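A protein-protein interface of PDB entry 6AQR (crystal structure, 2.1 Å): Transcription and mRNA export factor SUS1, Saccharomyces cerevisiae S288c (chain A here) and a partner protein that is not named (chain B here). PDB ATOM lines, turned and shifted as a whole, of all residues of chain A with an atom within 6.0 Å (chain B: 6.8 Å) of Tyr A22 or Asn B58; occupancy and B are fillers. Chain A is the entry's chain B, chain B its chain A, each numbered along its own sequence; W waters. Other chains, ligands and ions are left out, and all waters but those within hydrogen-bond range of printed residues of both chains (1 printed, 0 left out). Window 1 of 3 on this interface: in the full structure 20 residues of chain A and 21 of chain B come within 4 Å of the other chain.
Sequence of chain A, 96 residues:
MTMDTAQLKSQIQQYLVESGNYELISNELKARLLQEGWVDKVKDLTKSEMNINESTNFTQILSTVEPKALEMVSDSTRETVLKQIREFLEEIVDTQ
Of chain B, only Phe B45, Ile B57 and Asn B58 come within 4 Å of Tyr A22.
Asn B58 touches just one residue of chain A: Tyr A22 (2.7 Å).
Of the printed residues of chain A, Ile B57 touches Gln A13, Val A17 and Tyr A22.
Printed residues of chain B within 4 Å of Val A17: Phe B45 and Ile B57.
Printed residues of chain A within 4 Å of Phe B45: Val A17 (3.9 Å), Tyr A22 (3.6 Å) and Glu A23 (3.9 Å).
Printed residues of chain A within 4 Å of Glu B56: Gln A13.
Of the printed residues of chain B, Gln A13 touches Glu B56 and Ile B57.
The nearest residue of chain A that does not touch Asn B58 is Ser A26 (5.5 Å).
Printed residues of chain A that touch a printed residue of chain B: Gln A13, Val A17, Tyr A22 and Glu A23.
Printed residues of chain B that touch a printed residue of chain A: Phe B45, Glu B56, Ile B57 and Asn B58.
Water W1 lies within hydrogen-bond range of the side-chain amide nitrogen (ND2) of Asn B58 (2.8 Å) and the side-chain hydroxyl (OG) of Ser A26 (3.0 Å).
O of Met B49 is in hydrogen-bond range of N of Asn B58 (3.0 Å).
N of Cys B51 sits at hydrogen-bond distance from O of Glu B56 (3.1 Å).
The backbone NH (N) of Tyr A22 sits at hydrogen-bond distance from the backbone carbonyl oxygen (O) of Leu A16 (2.9 Å).
ND2 of Asn A27 sits close to O of Glu A23, 3.1 Å away.
N of Ile B57 lies within hydrogen-bond range of OE1 of Gln A13, at 2.7 Å.
The side-chain amide nitrogen of Asn B58 lies within hydrogen-bond range of the side-chain hydroxyl of Tyr A22 (2.7 Å).
Gln A13 touches Glu B56 (OE1 to CA, 3.0 Å).
CG1 of Val A17 touches CB of Phe B45, 3.9 Å away.
CG2 of Val A17 touches CD1 of Ile B57, at 3.5 Å.
Phe B45 touches Tyr A22 (CE2 to CE1, 3.6 Å).
Tyr A22 touches Ile B57.
CE1 of Phe B45 touches CG of Glu A23, at 3.9 Å.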
ATOM      1  N   GLN A  13     -23.352  -2.764 -18.823  1.00  0.00           N
ATOM      2  CA  GLN A  13     -22.590  -1.863 -19.714  1.00  0.00           C
ATOM      3  C   GLN A  13     -22.832  -2.208 -21.150  1.00  0.00           C
ATOM      4  O   GLN A  13     -23.074  -1.303 -21.968  1.00  0.00           O
ATOM      5  CB  GLN A  13     -21.096  -1.891 -19.446  1.00  0.00           C
ATOM      6  CG  GLN A  13     -20.683  -1.088 -18.240  1.00  0.00           C
ATOM      7  CD  GLN A  13     -19.312  -1.506 -17.731  1.00  0.00           C
ATOM      8  OE1 GLN A  13     -18.631  -2.342 -18.319  1.00  0.00           O
ATOM      9  NE2 GLN A  13     -18.910  -0.928 -16.608  1.00  0.00           N
ATOM     10  N   LEU A  16     -26.070  -0.934 -22.201  1.00  0.00           N
ATOM     11  CA  LEU A  16     -26.163   0.515 -22.336  1.00  0.00           C
ATOM     12  C   LEU A  16     -25.531   0.912 -23.686  1.00  0.00           C
ATOM     13  O   LEU A  16     -26.055   1.796 -24.343  1.00  0.00           O
ATOM     14  CB  LEU A  16     -25.475   1.227 -21.172  1.00  0.00           C
ATOM     15  CG  LEU A  16     -26.245   1.213 -19.841  1.00  0.00           C
ATOM     16  CD1 LEU A  16     -25.406   1.894 -18.768  1.00  0.00           C
ATOM     17  CD2 LEU A  16     -27.575   1.917 -19.996  1.00  0.00           C
ATOM     18  N   VAL A  17     -24.452   0.210 -24.095  1.00  0.00           N
ATOM     19  CA  VAL A  17     -23.828   0.438 -25.397  1.00  0.00           C
ATOM     20  C   VAL A  17     -24.760   0.050 -26.590  1.00  0.00           C
ATOM     21  O   VAL A  17     -25.035   0.888 -27.477  1.00  0.00           O
ATOM     22  CB  VAL A  17     -22.445  -0.225 -25.531  1.00  0.00           C
ATOM     23  CG1 VAL A  17     -21.913   0.096 -26.929  1.00  0.00           C
ATOM     24  CG2 VAL A  17     -21.473   0.281 -24.422  1.00  0.00           C
ATOM     25  N   SER A  19     -27.940  -0.182 -26.733  1.00  0.00           N
ATOM     26  CA  SER A  19     -29.171   0.573 -26.814  1.00  0.00           C
ATOM     27  C   SER A  19     -28.911   2.024 -27.249  1.00  0.00           C
ATOM     28  O   SER A  19     -29.862   2.785 -27.421  1.00  0.00           O
ATOM     29  CB  SER A  19     -29.942   0.515 -25.493  1.00  0.00           C
ATOM     30  OG  SER A  19     -29.222   1.140 -24.430  1.00  0.00           O
ATOM     31  N   GLY A  20     -27.632   2.414 -27.393  1.00  0.00           N
ATOM     32  CA  GLY A  20     -27.304   3.790 -27.625  1.00  0.00           C
ATOM     33  C   GLY A  20     -27.252   4.670 -26.408  1.00  0.00           C
ATOM     34  O   GLY A  20     -26.850   5.805 -26.528  1.00  0.00           O
ATOM     35  N   ASN A  21     -27.621   4.171 -25.218  1.00  0.00           N
ATOM     36  CA  ASN A  21     -27.703   5.063 -24.025  1.00  0.00           C
ATOM     37  C   ASN A  21     -26.302   5.369 -23.434  1.00  0.00           C
ATOM     38  O   ASN A  21     -26.093   6.369 -22.788  1.00  0.00           O
ATOM     39  CB  ASN A  21     -28.697   4.505 -22.969  1.00  0.00           C
ATOM     40  CG  ASN A  21     -30.142   4.419 -23.541  1.00  0.00           C
ATOM     41  OD1 ASN A  21     -30.836   3.471 -23.341  1.00  0.00           O
ATOM     42  ND2 ASN A  21     -30.519   5.386 -24.328  1.00  0.00           N
ATOM     43  N   TYR A  22     -25.365   4.497 -23.693  1.00  0.00           N
ATOM     44  CA  TYR A  22     -24.013   4.749 -23.242  1.00  0.00           C
ATOM     45  C   TYR A  22     -23.417   5.988 -23.884  1.00  0.00           C
ATOM     46  O   TYR A  22     -22.852   6.813 -23.187  1.00  0.00           O
ATOM     47  CB  TYR A  22     -23.133   3.516 -23.422  1.00  0.00           C
ATOM     48  CG  TYR A  22     -21.843   3.549 -22.570  1.00  0.00           C
ATOM     49  CD1 TYR A  22     -20.646   4.011 -23.109  1.00  0.00           C
ATOM     50  CD2 TYR A  22     -21.827   3.091 -21.252  1.00  0.00           C
ATOM     51  CE1 TYR A  22     -19.451   4.013 -22.352  1.00  0.00           C
ATOM     52  CE2 TYR A  22     -20.655   3.105 -20.480  1.00  0.00           C
ATOM     53  CZ  TYR A  22     -19.469   3.561 -21.030  1.00  0.00           C
ATOM     54  OH  TYR A  22     -18.343   3.582 -20.247  1.00  0.00           O
ATOM     55  N   GLU A  23     -23.602   6.149 -25.196  1.00  0.00           N
ATOM     56  CA  GLU A  23     -23.098   7.337 -25.912  1.00  0.00           C
ATOM     57  C   GLU A  23     -23.776   8.589 -25.367  1.00  0.00           C
ATOM     58  O   GLU A  23     -23.127   9.634 -25.263  1.00  0.00           O
ATOM     59  CB  GLU A  23     -23.355   7.281 -27.426  1.00  0.00           C
ATOM     60  CG  GLU A  23     -22.757   6.106 -28.166  1.00  0.00           C
ATOM     61  CD  GLU A  23     -23.755   5.490 -29.174  1.00  0.00           C
ATOM     62  OE1 GLU A  23     -24.313   4.385 -28.907  1.00  0.00           O
ATOM     63  OE2 GLU A  23     -23.988   6.132 -30.223  1.00  0.00           O
ATOM     64  N   LEU A  24     -25.071   8.479 -25.056  1.00  0.00           N
ATOM     65  CA  LEU A  24     -25.797   9.629 -24.484  1.00  0.00           C
ATOM     66  C   LEU A  24     -25.222  10.026 -23.113  1.00  0.00           C
ATOM     67  O   LEU A  24     -25.084  11.194 -22.847  1.00  0.00           O
ATOM     68  CB  LEU A  24     -27.297   9.374 -24.353  1.00  0.00           C
ATOM     69  CG  LEU A  24     -28.177   9.207 -25.635  1.00  0.00           C
ATOM     70  CD1 LEU A  24     -29.636   8.836 -25.252  1.00  0.00           C
ATOM     71  CD2 LEU A  24     -28.162  10.397 -26.616  1.00  0.00           C
ATOM     72  N   ILE A  25     -24.923   9.053 -22.256  1.00  0.00           N
ATOM     73  CA  ILE A  25     -24.331   9.320 -20.931  1.00  0.00           C
ATOM     74  C   ILE A  25     -22.948   9.942 -21.110  1.00  0.00           C
ATOM     75  O   ILE A  25     -22.647  11.004 -20.599  1.00  0.00           O
ATOM     76  CB  ILE A  25     -24.256   8.017 -20.066  1.00  0.00           C
ATOM     77  CG1 ILE A  25     -25.659   7.489 -19.747  1.00  0.00           C
ATOM     78  CG2 ILE A  25     -23.543   8.312 -18.749  1.00  0.00           C
ATOM     79  CD1 ILE A  25     -25.651   5.988 -19.471  1.00  0.00           C
ATOM     80  N   SER A  26     -22.160   9.305 -21.933  1.00  0.00           N
ATOM     81  CA  SER A  26     -20.795   9.702 -22.169  1.00  0.00           C
ATOM     82  C   SER A  26     -20.696  11.095 -22.809  1.00  0.00           C
ATOM     83  O   SER A  26     -19.993  11.973 -22.288  1.00  0.00           O
ATOM     84  CB  SER A  26     -20.113   8.624 -22.991  1.00  0.00           C
ATOM     85  OG  SER A  26     -18.751   8.963 -23.133  1.00  0.00           O
ATOM     86  N   ASN A  27     -21.511  11.376 -23.808  1.00  0.00           N
ATOM     87  CA  ASN A  27     -21.569  12.769 -24.347  1.00  0.00           C
ATOM     88  C   ASN A  27     -22.024  13.881 -23.447  1.00  0.00           C
ATOM     89  O   ASN A  27     -21.486  14.974 -23.457  1.00  0.00           O
ATOM     90  CB  ASN A  27     -22.373  12.809 -25.635  1.00  0.00           C
ATOM     91  CG  ASN A  27     -21.726  11.994 -26.701  1.00  0.00           C
ATOM     92  OD1 ASN A  27     -20.500  11.705 -26.666  1.00  0.00           O
ATOM     93  ND2 ASN A  27     -22.529  11.568 -27.630  1.00  0.00           N
ATOM     94  N   PHE A  88     -31.675   5.137 -16.809  1.00  0.00           N
ATOM     95  CA  PHE A  88     -31.385   4.043 -17.737  1.00  0.00           C
ATOM     96  C   PHE A  88     -31.361   2.676 -17.081  1.00  0.00           C
ATOM     97  O   PHE A  88     -31.807   1.690 -17.689  1.00  0.00           O
ATOM     98  CB  PHE A  88     -30.146   4.282 -18.623  1.00  0.00           C
ATOM     99  CG  PHE A  88     -30.309   5.424 -19.584  1.00  0.00           C
ATOM    100  CD1 PHE A  88     -31.463   5.567 -20.324  1.00  0.00           C
ATOM    101  CD2 PHE A  88     -29.306   6.381 -19.728  1.00  0.00           C
ATOM    102  CE1 PHE A  88     -31.619   6.631 -21.201  1.00  0.00           C
ATOM    103  CE2 PHE A  88     -29.449   7.453 -20.594  1.00  0.00           C
ATOM    104  CZ  PHE A  88     -30.607   7.575 -21.343  1.00  0.00           C
ATOM    105  N   PHE B  45     -16.707   1.298 -28.780  1.00  0.00           N
ATOM    106  CA  PHE B  45     -16.881   0.839 -27.389  1.00  0.00           C
ATOM    107  C   PHE B  45     -16.745  -0.687 -27.199  1.00  0.00           C
ATOM    108  O   PHE B  45     -16.003  -1.144 -26.327  1.00  0.00           O
ATOM    109  CB  PHE B  45     -18.234   1.297 -26.813  1.00  0.00           C
ATOM    110  CG  PHE B  45     -18.287   2.758 -26.464  1.00  0.00           C
ATOM    111  CD1 PHE B  45     -19.258   3.539 -27.032  1.00  0.00           C
ATOM    112  CD2 PHE B  45     -17.384   3.373 -25.551  1.00  0.00           C
ATOM    113  CE1 PHE B  45     -19.326   4.921 -26.754  1.00  0.00           C
ATOM    114  CE2 PHE B  45     -17.451   4.764 -25.281  1.00  0.00           C
ATOM    115  CZ  PHE B  45     -18.431   5.534 -25.908  1.00  0.00           C
ATOM    116  N   MET B  49     -12.792  -0.623 -26.493  1.00  0.00           N
ATOM    117  CA  MET B  49     -12.831  -0.229 -25.108  1.00  0.00           C
ATOM    118  C   MET B  49     -13.387  -1.281 -24.111  1.00  0.00           C
ATOM    119  O   MET B  49     -13.812  -0.941 -23.010  1.00  0.00           O
ATOM    120  CB  MET B  49     -13.523   1.147 -24.971  1.00  0.00           C
ATOM    121  CG  MET B  49     -12.681   2.268 -25.585  1.00  0.00           C
ATOM    122  SD  MET B  49     -13.681   3.719 -25.909  1.00  0.00           S
ATOM    123  CE  MET B  49     -12.592   4.661 -27.019  1.00  0.00           C
ATOM    124  N   LYS B  50     -13.320  -2.551 -24.488  1.00  0.00           N
ATOM    125  CA  LYS B  50     -13.887  -3.581 -23.681  1.00  0.00           C
ATOM    126  C   LYS B  50     -12.762  -4.538 -23.298  1.00  0.00           C
ATOM    127  O   LYS B  50     -12.118  -5.074 -24.159  1.00  0.00           O
ATOM    128  CB  LYS B  50     -14.996  -4.293 -24.437  1.00  0.00           C
ATOM    129  CG  LYS B  50     -15.698  -5.362 -23.630  1.00  0.00           C
ATOM    130  CD  LYS B  50     -16.525  -6.218 -24.587  1.00  0.00           C
ATOM    131  CE  LYS B  50     -17.593  -6.971 -23.842  1.00  0.00           C
ATOM    132  NZ  LYS B  50     -18.168  -8.003 -24.769  1.00  0.00           N
ATOM    133  N   CYS B  51     -12.526  -4.727 -22.004  1.00  0.00           N
ATOM    134  CA  CYS B  51     -11.365  -5.541 -21.587  1.00  0.00           C
ATOM    135  C   CYS B  51     -11.643  -6.996 -21.940  1.00  0.00           C
ATOM    136  O   CYS B  51     -12.731  -7.467 -21.667  1.00  0.00           O
ATOM    137  CB  CYS B  51     -11.173  -5.430 -20.093  1.00  0.00           C
ATOM    138  SG  CYS B  51      -9.695  -6.213 -19.358  1.00  0.00           S
ATOM    139  N   GLU B  56     -15.524  -5.348 -18.838  1.00  0.00           N
ATOM    140  CA  GLU B  56     -16.122  -4.031 -18.617  1.00  0.00           C
ATOM    141  C   GLU B  56     -15.674  -3.015 -19.710  1.00  0.00           C
ATOM    142  O   GLU B  56     -14.559  -3.076 -20.313  1.00  0.00           O
ATOM    143  CB  GLU B  56     -15.752  -3.460 -17.248  1.00  0.00           C
ATOM    144  CG  GLU B  56     -16.080  -4.266 -16.011  1.00  0.00           C
ATOM    145  CD  GLU B  56     -15.705  -3.463 -14.787  1.00  0.00           C
ATOM    146  OE1 GLU B  56     -16.027  -2.255 -14.829  1.00  0.00           O
ATOM    147  OE2 GLU B  56     -15.057  -3.989 -13.827  1.00  0.00           O
ATOM    148  N   ILE B  57     -16.555  -2.072 -19.946  1.00  0.00           N
ATOM    149  CA  ILE B  57     -16.293  -1.003 -20.875  1.00  0.00           C
ATOM    150  C   ILE B  57     -15.712   0.142 -20.095  1.00  0.00           C
ATOM    151  O   ILE B  57     -16.218   0.482 -19.019  1.00  0.00           O
ATOM    152  CB  ILE B  57     -17.588  -0.648 -21.631  1.00  0.00           C
ATOM    153  CG1 ILE B  57     -17.913  -1.869 -22.543  1.00  0.00           C
ATOM    154  CG2 ILE B  57     -17.369   0.650 -22.442  1.00  0.00           C
ATOM    155  CD1 ILE B  57     -19.362  -2.005 -22.816  1.00  0.00           C
ATOM    156  N   ASN B  58     -14.625   0.726 -20.627  1.00  0.00           N
ATOM    157  CA  ASN B  58     -13.983   1.890 -19.995  1.00  0.00           C
ATOM    158  C   ASN B  58     -13.590   1.661 -18.536  1.00  0.00           C
ATOM    159  O   ASN B  58     -13.800   2.534 -17.672  1.00  0.00           O
ATOM    160  CB  ASN B  58     -14.883   3.124 -20.077  1.00  0.00           C
ATOM    161  CG  ASN B  58     -15.028   3.680 -21.480  1.00  0.00           C
ATOM    162  OD1 ASN B  58     -14.123   3.577 -22.329  1.00  0.00           O
ATOM    163  ND2 ASN B  58     -16.162   4.363 -21.704  1.00  0.00           N
ATOM    164  N   SER B  59     -12.982   0.517 -18.248  1.00  0.00           N
ATOM    165  CA  SER B  59     -12.387   0.269 -16.930  1.00  0.00           C
ATOM    166  C   SER B  59     -11.074   0.999 -16.860  1.00  0.00           C
ATOM    167  O   SER B  59      -9.970   0.385 -16.888  1.00  0.00           O
ATOM    168  CB  SER B  59     -12.201  -1.271 -16.729  1.00  0.00           C
ATOM    169  OG  SER B  59     -11.687  -1.540 -15.452  1.00  0.00           O
ATOM    170  N   GLY B  60     -11.169   2.334 -16.858  1.00  0.00           N
ATOM    171  CA  GLY B  60     -10.003   3.200 -17.222  1.00  0.00           C
ATOM    172  C   GLY B  60      -9.651   3.085 -18.731  1.00  0.00           C
ATOM    173  O   GLY B  60     -10.444   2.627 -19.527  1.00  0.00           O
ATOM    174  N   ALA B  61      -8.477   3.545 -19.109  1.00  0.00           N
ATOM    175  CA  ALA B  61      -8.007   3.373 -20.457  1.00  0.00           C
ATOM    176  C   ALA B  61      -7.987   1.878 -20.793  1.00  0.00           C
ATOM    177  O   ALA B  61      -7.666   1.075 -19.929  1.00  0.00           O
ATOM    178  CB  ALA B  61      -6.605   3.985 -20.635  1.00  0.00           C
ATOM    179  N   THR B  62      -8.325   1.536 -22.043  1.00  0.00           N
ATOM    180  CA  THR B  62      -8.187   0.177 -22.573  1.00  0.00           C
ATOM    181  C   THR B  62      -7.131   0.224 -23.624  1.00  0.00           C
ATOM    182  O   THR B  62      -7.152   1.132 -24.452  1.00  0.00           O
ATOM    183  CB  THR B  62      -9.533  -0.305 -23.161  1.00  0.00           C
ATOM    184  OG1 THR B  62     -10.605   0.002 -22.243  1.00  0.00           O
ATOM    185  CG2 THR B  62      -9.509  -1.800 -23.411  1.00  0.00           C
ATOM    186  N   CYS B  73      -7.749  -3.577 -19.807  1.00  0.00           N
ATOM    187  CA  CYS B  73      -7.967  -2.390 -19.049  1.00  0.00           C
ATOM    188  C   CYS B  73      -6.784  -1.926 -18.158  1.00  0.00           C
ATOM    189  O   CYS B  73      -5.842  -2.712 -17.821  1.00  0.00           O
ATOM    190  CB  CYS B  73      -9.229  -2.557 -18.178  1.00  0.00           C
ATOM    191  SG  CYS B  73      -9.106  -3.577 -16.645  1.00  0.00           S
ATOM    192  N   ASN B  75      -7.752  -0.090 -15.067  1.00  0.00           N
ATOM    193  CA  ASN B  75      -8.198   0.028 -13.653  1.00  0.00           C
ATOM    194  C   ASN B  75      -8.028  -1.264 -12.808  1.00  0.00           C
ATOM    195  O   ASN B  75      -7.772  -1.167 -11.625  1.00  0.00           O
ATOM    196  CB  ASN B  75      -9.631   0.578 -13.541  1.00  0.00           C
ATOM    197  CG  ASN B  75      -9.695   2.113 -13.715  1.00  0.00           C
ATOM    198  OD1 ASN B  75      -8.715   2.781 -14.073  1.00  0.00           O
ATOM    199  ND2 ASN B  75     -10.858   2.653 -13.528  1.00  0.00           N
ATOM    200  N   SER B  94      -6.832   3.128 -26.571  1.00  0.00           N
ATOM    201  CA  SER B  94      -7.860   3.244 -27.602  1.00  0.00           C
ATOM    202  C   SER B  94      -8.609   4.562 -27.595  1.00  0.00           C
ATOM    203  O   SER B  94      -9.509   4.722 -28.444  1.00  0.00           O
ATOM    204  CB  SER B  94      -8.859   2.132 -27.517  1.00  0.00           C
ATOM    205  OG  SER B  94      -9.530   2.114 -26.234  1.00  0.00           O
ATOM    206  N   ASN B  95      -8.273   5.480 -26.677  1.00  0.00           N
ATOM    207  CA  ASN B  95      -8.893   6.852 -26.686  1.00  0.00           C
ATOM    208  C   ASN B  95      -8.045   7.852 -27.448  1.00  0.00           C
ATOM    209  O   ASN B  95      -8.517   8.936 -27.792  1.00  0.00           O
ATOM    210  CB  ASN B  95      -9.072   7.420 -25.271  1.00  0.00           C
ATOM    211  CG  ASN B  95     -10.202   6.765 -24.502  1.00  0.00           C
ATOM    212  OD1 ASN B  95      -9.958   6.000 -23.591  1.00  0.00           O
ATOM    213  ND2 ASN B  95     -11.451   7.045 -24.885  1.00  0.00           N
HETATM  214  O   HOH W   1     -16.508   7.073 -22.473  1.00  0.00           O
